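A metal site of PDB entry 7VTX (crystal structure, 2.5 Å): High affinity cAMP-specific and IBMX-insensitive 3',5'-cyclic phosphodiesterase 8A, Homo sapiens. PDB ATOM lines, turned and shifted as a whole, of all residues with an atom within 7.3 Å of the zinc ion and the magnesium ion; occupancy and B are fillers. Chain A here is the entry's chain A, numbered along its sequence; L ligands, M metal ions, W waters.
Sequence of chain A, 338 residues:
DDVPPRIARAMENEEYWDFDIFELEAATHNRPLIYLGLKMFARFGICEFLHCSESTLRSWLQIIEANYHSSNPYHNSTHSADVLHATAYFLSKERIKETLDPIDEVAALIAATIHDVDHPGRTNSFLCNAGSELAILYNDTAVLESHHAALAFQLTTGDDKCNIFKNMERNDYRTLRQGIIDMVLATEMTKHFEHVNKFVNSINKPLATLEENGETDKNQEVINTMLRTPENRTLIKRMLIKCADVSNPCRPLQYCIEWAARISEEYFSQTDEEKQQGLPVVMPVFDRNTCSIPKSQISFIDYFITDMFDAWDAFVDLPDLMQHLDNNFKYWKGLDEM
N of Asp 116 is in hydrogen-bond range of OH of Tyr 68 (3.4 Å).
OH of Tyr 74 sits close to ND1 of His 79.
The backbone carbonyl oxygen of Ala 112 lies within hydrogen-bond range of a ring nitrogen (ND1) of His 115.
OD1 of Asp 245 sits close to NE2 of His 115, at 3.1 Å.
Within 4 Å of the zinc ion: His 79, His 115, Asp 116 and Asp 245.
One residue has an atom within 4 Å of the magnesium ion: Asp 116.
The nearest printed residue that does not touch the magnesium ion is Thr 187 (4.1 Å).
The zinc ion is bound by the side-chain carboxylate of Asp 116 (2.1 Å), the side-chain carboxylate of Asp 245 (2.1 Å), water W4 (2.2 Å), water W3 (2.4 Å) and a ring nitrogen (NE2) of His 79 (2.6 Å).
Slightly farther from the zinc ion lies NE2 of His 115 (2.6 Å).
Water W3 binds the magnesium ion (2.0 Å).
Water W1 is bound to the magnesium ion, at 2.0 Å.
Water W5 binds the magnesium ion, 2.1 Å away.
Water W2 is bound to the magnesium ion, at 2.1 Å.
OD1 of Asp 116 binds the magnesium ion (2.2 Å).
Water W5 lies within hydrogen-bond range of a ring nitrogen (NE2) of His 148 (2.9 Å) and the side-chain carboxylate (OE2) of Glu 145 (3.4 Å).
Water W1 bridges O of His 115 (2.8 Å) and OG1 of Thr 187 (2.8 Å).
Water W2 lies within hydrogen-bond range of OE2 of Glu 145 (2.7 Å) and O of Thr 187 (3.2 Å).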
ATOM      1  N   TYR A  68       1.998 -12.209  -4.041  1.00  0.00           N
ATOM      2  CA  TYR A  68       0.857 -12.748  -3.279  1.00  0.00           C
ATOM      3  C   TYR A  68       0.451 -14.099  -3.865  1.00  0.00           C
ATOM      4  O   TYR A  68       0.249 -14.220  -5.071  1.00  0.00           O
ATOM      5  CB  TYR A  68      -0.342 -11.803  -3.283  1.00  0.00           C
ATOM      6  CG  TYR A  68      -0.254 -10.699  -2.261  1.00  0.00           C
ATOM      7  CD1 TYR A  68       0.434  -9.528  -2.533  1.00  0.00           C
ATOM      8  CD2 TYR A  68      -0.847 -10.836  -1.000  1.00  0.00           C
ATOM      9  CE1 TYR A  68       0.538  -8.513  -1.589  1.00  0.00           C
ATOM     10  CE2 TYR A  68      -0.750  -9.826  -0.045  1.00  0.00           C
ATOM     11  CZ  TYR A  68      -0.056  -8.671  -0.354  1.00  0.00           C
ATOM     12  OH  TYR A  68       0.045  -7.651   0.573  1.00  0.00           O
ATOM     13  N   TYR A  74      -7.447 -17.045   1.808  1.00  0.00           N
ATOM     14  CA  TYR A  74      -7.644 -15.705   2.381  1.00  0.00           C
ATOM     15  C   TYR A  74      -6.471 -14.773   2.068  1.00  0.00           C
ATOM     16  O   TYR A  74      -6.673 -13.702   1.477  1.00  0.00           O
ATOM     17  CB  TYR A  74      -7.839 -15.809   3.893  1.00  0.00           C
ATOM     18  CG  TYR A  74      -8.102 -14.504   4.612  1.00  0.00           C
ATOM     19  CD1 TYR A  74      -9.395 -14.022   4.783  1.00  0.00           C
ATOM     20  CD2 TYR A  74      -7.048 -13.768   5.157  1.00  0.00           C
ATOM     21  CE1 TYR A  74      -9.647 -12.833   5.471  1.00  0.00           C
ATOM     22  CE2 TYR A  74      -7.284 -12.576   5.838  1.00  0.00           C
ATOM     23  CZ  TYR A  74      -8.582 -12.110   5.990  1.00  0.00           C
ATOM     24  OH  TYR A  74      -8.807 -10.945   6.666  1.00  0.00           O
ATOM     25  N   HIS A  75      -5.261 -15.169   2.468  1.00  0.00           N
ATOM     26  CA  HIS A  75      -4.071 -14.314   2.323  1.00  0.00           C
ATOM     27  C   HIS A  75      -3.519 -14.309   0.883  1.00  0.00           C
ATOM     28  O   HIS A  75      -2.417 -14.797   0.621  1.00  0.00           O
ATOM     29  CB  HIS A  75      -2.973 -14.701   3.333  1.00  0.00           C
ATOM     30  CG  HIS A  75      -3.299 -14.334   4.738  1.00  0.00           C
ATOM     31  ND1 HIS A  75      -3.431 -15.252   5.745  1.00  0.00           N
ATOM     32  CD2 HIS A  75      -3.542 -13.128   5.300  1.00  0.00           C
ATOM     33  CE1 HIS A  75      -3.734 -14.638   6.876  1.00  0.00           C
ATOM     34  NE2 HIS A  75      -3.810 -13.343   6.633  1.00  0.00           N
ATOM     35  N   HIS A  79      -7.139  -9.888  -0.415  1.00  0.00           N
ATOM     36  CA  HIS A  79      -7.054  -9.407   0.964  1.00  0.00           C
ATOM     37  C   HIS A  79      -6.354  -8.059   1.052  1.00  0.00           C
ATOM     38  O   HIS A  79      -6.822  -7.159   1.735  1.00  0.00           O
ATOM     39  CB  HIS A  79      -6.342 -10.407   1.883  1.00  0.00           C
ATOM     40  CG  HIS A  79      -6.171  -9.904   3.275  1.00  0.00           C
ATOM     41  ND1 HIS A  79      -7.239  -9.620   4.091  1.00  0.00           N
ATOM     42  CD2 HIS A  79      -5.064  -9.582   3.984  1.00  0.00           C
ATOM     43  CE1 HIS A  79      -6.802  -9.168   5.251  1.00  0.00           C
ATOM     44  NE2 HIS A  79      -5.484  -9.140   5.213  1.00  0.00           N
ATOM     45  N   SER A  80      -5.222  -7.932   0.377  1.00  0.00           N
ATOM     46  CA  SER A  80      -4.438  -6.699   0.380  1.00  0.00           C
ATOM     47  C   SER A  80      -5.221  -5.522  -0.191  1.00  0.00           C
ATOM     48  O   SER A  80      -5.172  -4.420   0.346  1.00  0.00           O
ATOM     49  CB  SER A  80      -3.121  -6.889  -0.389  1.00  0.00           C
ATOM     50  OG  SER A  80      -2.401  -5.675  -0.488  1.00  0.00           O
ATOM     51  N   VAL A  83      -7.861  -4.640   2.374  1.00  0.00           N
ATOM     52  CA  VAL A  83      -7.202  -3.908   3.461  1.00  0.00           C
ATOM     53  C   VAL A  83      -6.768  -2.504   2.995  1.00  0.00           C
ATOM     54  O   VAL A  83      -6.817  -1.558   3.775  1.00  0.00           O
ATOM     55  CB  VAL A  83      -6.015  -4.707   4.047  1.00  0.00           C
ATOM     56  CG1 VAL A  83      -5.203  -3.884   5.032  1.00  0.00           C
ATOM     57  CG2 VAL A  83      -6.549  -5.950   4.735  1.00  0.00           C
ATOM     58  N   ALA A 112      -0.549  -0.946   3.725  1.00  0.00           N
ATOM     59  CA  ALA A 112      -1.708  -1.786   3.406  1.00  0.00           C
ATOM     60  C   ALA A 112      -1.458  -2.681   2.193  1.00  0.00           C
ATOM     61  O   ALA A 112      -1.791  -3.865   2.202  1.00  0.00           O
ATOM     62  CB  ALA A 112      -2.939  -0.917   3.175  1.00  0.00           C
ATOM     63  N   HIS A 115       1.565  -5.296   3.326  1.00  0.00           N
ATOM     64  CA  HIS A 115       1.596  -5.916   4.671  1.00  0.00           C
ATOM     65  C   HIS A 115       1.600  -7.440   4.749  1.00  0.00           C
ATOM     66  O   HIS A 115       2.082  -7.972   5.736  1.00  0.00           O
ATOM     67  CB  HIS A 115       0.490  -5.356   5.593  1.00  0.00           C
ATOM     68  CG  HIS A 115      -0.883  -5.874   5.293  1.00  0.00           C
ATOM     69  ND1 HIS A 115      -1.516  -5.651   4.098  1.00  0.00           N
ATOM     70  CD2 HIS A 115      -1.739  -6.598   6.045  1.00  0.00           C
ATOM     71  CE1 HIS A 115      -2.707  -6.218   4.119  1.00  0.00           C
ATOM     72  NE2 HIS A 115      -2.864  -6.798   5.290  1.00  0.00           N
ATOM     73  N   ASP A 116       1.050  -8.131   3.748  1.00  0.00           N
ATOM     74  CA  ASP A 116       1.028  -9.599   3.713  1.00  0.00           C
ATOM     75  C   ASP A 116       1.701 -10.206   2.472  1.00  0.00           C
ATOM     76  O   ASP A 116       1.345 -11.308   2.056  1.00  0.00           O
ATOM     77  CB  ASP A 116      -0.429 -10.096   3.811  1.00  0.00           C
ATOM     78  CG  ASP A 116      -0.944 -10.166   5.228  1.00  0.00           C
ATOM     79  OD1 ASP A 116      -0.153 -10.159   6.192  1.00  0.00           O
ATOM     80  OD2 ASP A 116      -2.175 -10.266   5.388  1.00  0.00           O
ATOM     81  N   VAL A 117       2.671  -9.510   1.892  1.00  0.00           N
ATOM     82  CA  VAL A 117       3.332 -10.008   0.663  1.00  0.00           C
ATOM     83  C   VAL A 117       4.125 -11.301   0.936  1.00  0.00           C
ATOM     84  O   VAL A 117       4.876 -11.389   1.908  1.00  0.00           O
ATOM     85  CB  VAL A 117       4.230  -8.921  -0.006  1.00  0.00           C
ATOM     86  CG1 VAL A 117       5.451  -8.584   0.840  1.00  0.00           C
ATOM     87  CG2 VAL A 117       4.634  -9.354  -1.403  1.00  0.00           C
ATOM     88  N   HIS A 119       2.850 -14.274   1.849  1.00  0.00           N
ATOM     89  CA  HIS A 119       2.257 -15.022   2.968  1.00  0.00           C
ATOM     90  C   HIS A 119       2.087 -16.477   2.488  1.00  0.00           C
ATOM     91  O   HIS A 119       1.541 -16.685   1.408  1.00  0.00           O
ATOM     92  CB  HIS A 119       0.890 -14.402   3.324  1.00  0.00           C
ATOM     93  CG  HIS A 119       0.428 -14.616   4.730  1.00  0.00           C
ATOM     94  ND1 HIS A 119       0.169 -15.865   5.250  1.00  0.00           N
ATOM     95  CD2 HIS A 119       0.115 -13.734   5.706  1.00  0.00           C
ATOM     96  CE1 HIS A 119      -0.251 -15.749   6.504  1.00  0.00           C
ATOM     97  NE2 HIS A 119      -0.293 -14.463   6.798  1.00  0.00           N
ATOM     98  N   LEU A 144       6.698 -13.574   9.881  1.00  0.00           N
ATOM     99  CA  LEU A 144       6.081 -13.185   8.607  1.00  0.00           C
ATOM    100  C   LEU A 144       6.019 -11.676   8.440  1.00  0.00           C
ATOM    101  O   LEU A 144       6.242 -11.180   7.340  1.00  0.00           O
ATOM    102  CB  LEU A 144       4.696 -13.820   8.458  1.00  0.00           C
ATOM    103  CG  LEU A 144       4.742 -15.340   8.227  1.00  0.00           C
ATOM    104  CD1 LEU A 144       3.395 -15.978   8.518  1.00  0.00           C
ATOM    105  CD2 LEU A 144       5.219 -15.677   6.823  1.00  0.00           C
ATOM    106  N   GLU A 145       5.739 -10.962   9.530  1.00  0.00           N
ATOM    107  CA  GLU A 145       5.633  -9.494   9.485  1.00  0.00           C
ATOM    108  C   GLU A 145       6.962  -8.863   9.069  1.00  0.00           C
ATOM    109  O   GLU A 145       6.978  -7.938   8.250  1.00  0.00           O
ATOM    110  CB  GLU A 145       5.193  -8.909  10.837  1.00  0.00           C
ATOM    111  CG  GLU A 145       3.730  -9.162  11.193  1.00  0.00           C
ATOM    112  CD  GLU A 145       3.453 -10.555  11.732  1.00  0.00           C
ATOM    113  OE1 GLU A 145       4.388 -11.207  12.255  1.00  0.00           O
ATOM    114  OE2 GLU A 145       2.301 -11.010  11.640  1.00  0.00           O
ATOM    115  N   HIS A 148       7.359  -9.816   5.250  1.00  0.00           N
ATOM    116  CA  HIS A 148       6.489  -8.998   4.393  1.00  0.00           C
ATOM    117  C   HIS A 148       7.154  -7.648   4.103  1.00  0.00           C
ATOM    118  O   HIS A 148       7.290  -7.256   2.947  1.00  0.00           O
ATOM    119  CB  HIS A 148       5.117  -8.758   5.040  1.00  0.00           C
ATOM    120  CG  HIS A 148       4.358 -10.005   5.344  1.00  0.00           C
ATOM    121  ND1 HIS A 148       4.326 -11.092   4.506  1.00  0.00           N
ATOM    122  CD2 HIS A 148       3.587 -10.336   6.412  1.00  0.00           C
ATOM    123  CE1 HIS A 148       3.582 -12.046   5.039  1.00  0.00           C
ATOM    124  NE2 HIS A 148       3.120 -11.608   6.192  1.00  0.00           N
ATOM    125  N   VAL A 184       3.530  -2.203   9.191  1.00  0.00           N
ATOM    126  CA  VAL A 184       3.572  -3.617   8.794  1.00  0.00           C
ATOM    127  C   VAL A 184       3.889  -4.520   9.987  1.00  0.00           C
ATOM    128  O   VAL A 184       3.269  -5.574  10.155  1.00  0.00           O
ATOM    129  CB  VAL A 184       4.565  -3.883   7.636  1.00  0.00           C
ATOM    130  CG1 VAL A 184       4.681  -5.383   7.340  1.00  0.00           C
ATOM    131  CG2 VAL A 184       4.109  -3.160   6.380  1.00  0.00           C
ATOM    132  N   THR A 187       0.952  -5.134  12.654  1.00  0.00           N
ATOM    133  CA  THR A 187      -0.088  -6.132  12.371  1.00  0.00           C
ATOM    134  C   THR A 187       0.128  -7.508  13.054  1.00  0.00           C
ATOM    135  O   THR A 187      -0.756  -8.362  12.993  1.00  0.00           O
ATOM    136  CB  THR A 187      -0.219  -6.383  10.854  1.00  0.00           C
ATOM    137  OG1 THR A 187       1.002  -6.915  10.341  1.00  0.00           O
ATOM    138  CG2 THR A 187      -0.582  -5.088  10.126  1.00  0.00           C
ATOM    139  N   GLU A 188       1.281  -7.721  13.685  1.00  0.00           N
ATOM    140  CA  GLU A 188       1.547  -8.982  14.390  1.00  0.00           C
ATOM    141  C   GLU A 188       0.530  -9.215  15.505  1.00  0.00           C
ATOM    142  O   GLU A 188       0.347  -8.361  16.371  1.00  0.00           O
ATOM    143  CB  GLU A 188       2.982  -9.021  14.955  1.00  0.00           C
ATOM    144  CG  GLU A 188       3.393 -10.407  15.450  1.00  0.00           C
ATOM    145  CD  GLU A 188       4.763 -10.450  16.098  1.00  0.00           C
ATOM    146  OE1 GLU A 188       5.356  -9.373  16.352  1.00  0.00           O
ATOM    147  OE2 GLU A 188       5.247 -11.559  16.385  1.00  0.00           O
ATOM    148  N   MET A 189      -0.111 -10.379  15.481  1.00  0.00           N
ATOM    149  CA  MET A 189      -1.193 -10.732  16.402  1.00  0.00           C
ATOM    150  C   MET A 189      -0.805 -10.635  17.881  1.00  0.00           C
ATOM    151  O   MET A 189      -1.609 -10.198  18.706  1.00  0.00           O
ATOM    152  CB  MET A 189      -1.757 -12.119  16.031  1.00  0.00           C
ATOM    153  CG  MET A 189      -2.703 -12.791  17.019  1.00  0.00           C
ATOM    154  SD  MET A 189      -1.811 -13.968  18.070  1.00  0.00           S
ATOM    155  CE  MET A 189      -3.143 -14.909  18.814  1.00  0.00           C
ATOM    156  N   ILE A 241      -3.995   0.724  10.681  1.00  0.00           N
ATOM    157  CA  ILE A 241      -3.569  -0.480   9.956  1.00  0.00           C
ATOM    158  C   ILE A 241      -4.161  -1.745  10.595  1.00  0.00           C
ATOM    159  O   ILE A 241      -4.521  -2.687   9.889  1.00  0.00           O
ATOM    160  CB  ILE A 241      -2.019  -0.572   9.827  1.00  0.00           C
ATOM    161  CG1 ILE A 241      -1.583  -1.619   8.784  1.00  0.00           C
ATOM    162  CG2 ILE A 241      -1.345  -0.877  11.166  1.00  0.00           C
ATOM    163  CD1 ILE A 241      -1.740  -1.170   7.352  1.00  0.00           C
ATOM    164  N   ALA A 244      -8.058  -1.810   9.745  1.00  0.00           N
ATOM    165  CA  ALA A 244      -8.199  -2.147   8.315  1.00  0.00           C
ATOM    166  C   ALA A 244      -7.856  -3.607   8.024  1.00  0.00           C
ATOM    167  O   ALA A 244      -8.551  -4.249   7.236  1.00  0.00           O
ATOM    168  CB  ALA A 244      -7.341  -1.218   7.458  1.00  0.00           C
ATOM    169  N   ASP A 245      -6.798  -4.126   8.651  1.00  0.00           N
ATOM    170  CA  ASP A 245      -6.401  -5.512   8.453  1.00  0.00           C
ATOM    171  C   ASP A 245      -7.523  -6.508   8.760  1.00  0.00           C
ATOM    172  O   ASP A 245      -7.699  -7.479   8.017  1.00  0.00           O
ATOM    173  CB  ASP A 245      -5.165  -5.878   9.282  1.00  0.00           C
ATOM    174  CG  ASP A 245      -4.651  -7.287   8.978  1.00  0.00           C
ATOM    175  OD1 ASP A 245      -4.449  -7.598   7.792  1.00  0.00           O
ATOM    176  OD2 ASP A 245      -4.472  -8.087   9.913  1.00  0.00           O
ATOM    177  N   VAL A 246      -8.264  -6.280   9.854  1.00  0.00           N
ATOM    178  CA  VAL A 246      -9.355  -7.168  10.264  1.00  0.00           C
ATOM    179  C   VAL A 246     -10.732  -6.479  10.231  1.00  0.00           C
ATOM    180  O   VAL A 246     -11.542  -6.637  11.132  1.00  0.00           O
ATOM    181  CB  VAL A 246      -9.065  -7.812  11.649  1.00  0.00           C
ATOM    182  CG1 VAL A 246      -7.813  -8.671  11.571  1.00  0.00           C
ATOM    183  CG2 VAL A 246      -8.903  -6.779  12.752  1.00  0.00           C
HETATM  184  N1  LIG L   1     -11.793 -14.858  11.736  1.00  0.00           N
HETATM  185  C1  LIG L   1      -8.861 -12.074   9.936  1.00  0.00           C
HETATM  186  C2  LIG L   1     -10.526 -13.199  10.619  1.00  0.00           C
HETATM  187  C3  LIG L   1     -11.776 -13.768  10.940  1.00  0.00           C
HETATM  188  N2  LIG L   1      -9.396 -14.865  11.965  1.00  0.00           N
HETATM  189  C4  LIG L   1      -9.407 -13.786  11.174  1.00  0.00           C
HETATM  190  C5  LIG L   1     -10.625 -15.312  12.184  1.00  0.00           C
HETATM  191  N3  LIG L   1      -8.340 -13.051  10.724  1.00  0.00           N
HETATM  192  N4  LIG L   1     -10.169 -12.112   9.838  1.00  0.00           N
HETATM  193  N5  LIG L   1     -12.943 -13.293  10.518  1.00  0.00           N
HETATM  194 CL1  LIG L   1     -10.731 -16.698  13.216  1.00  0.00          CL
HETATM  195  C6  LIG L   1      -6.931 -13.286  11.043  1.00  0.00           C
HETATM  196  C7  LIG L   1      -6.612 -13.082  12.509  1.00  0.00           C
HETATM  197  C8  LIG L   1      -6.313 -11.812  12.995  1.00  0.00           C
HETATM  198  C9  LIG L   1      -6.127 -11.638  14.358  1.00  0.00           C
HETATM  199  C10 LIG L   1      -6.230 -12.699  15.247  1.00  0.00           C
HETATM  200  C11 LIG L   1      -6.515 -13.980  14.773  1.00  0.00           C
HETATM  201  C12 LIG L   1      -6.691 -14.154  13.390  1.00  0.00           C
HETATM  202  O1  LIG L   1      -5.850 -10.510  15.100  1.00  0.00           O
HETATM  203  C13 LIG L   1      -5.740  -9.224  14.460  1.00  0.00           C
HETATM  204  C14 LIG L   1      -4.315  -8.766  14.910  1.00  0.00           C
HETATM  205  F1  LIG L   1      -4.162  -8.925  16.251  1.00  0.00           F
HETATM  206  F2  LIG L   1      -3.375  -9.558  14.326  1.00  0.00           F
HETATM  207  C15 LIG L   1      -6.701 -15.124  15.693  1.00  0.00           C
HETATM  208  C16 LIG L   1      -5.949 -15.254  16.855  1.00  0.00           C
HETATM  209  C17 LIG L   1      -6.167 -16.327  17.701  1.00  0.00           C
HETATM  210  N6  LIG L   1      -7.079 -17.270  17.469  1.00  0.00           N
HETATM  211  C18 LIG L   1      -7.813 -17.150  16.356  1.00  0.00           C
HETATM  212  C19 LIG L   1      -7.663 -16.107  15.461  1.00  0.00           C
HETATM  213 ZN    ZN M   1      -3.348  -9.006   6.630  1.00  0.00          ZN
HETATM  214 MG    MG M   2      -0.124 -10.268   8.357  1.00  0.00          MG
HETATM  215  O   HOH W   1       1.249  -8.767   8.246  1.00  0.00           O
HETATM  216  O   HOH W   2      -0.013 -10.147  10.463  1.00  0.00           O
HETATM  217  O   HOH W   3      -1.711  -9.061   8.364  1.00  0.00           O
HETATM  218  O   HOH W   4      -4.504 -10.752   7.166  1.00  0.00           O
HETATM  219  O   HOH W   5       1.353 -11.725   8.456  1.00  0.00           O
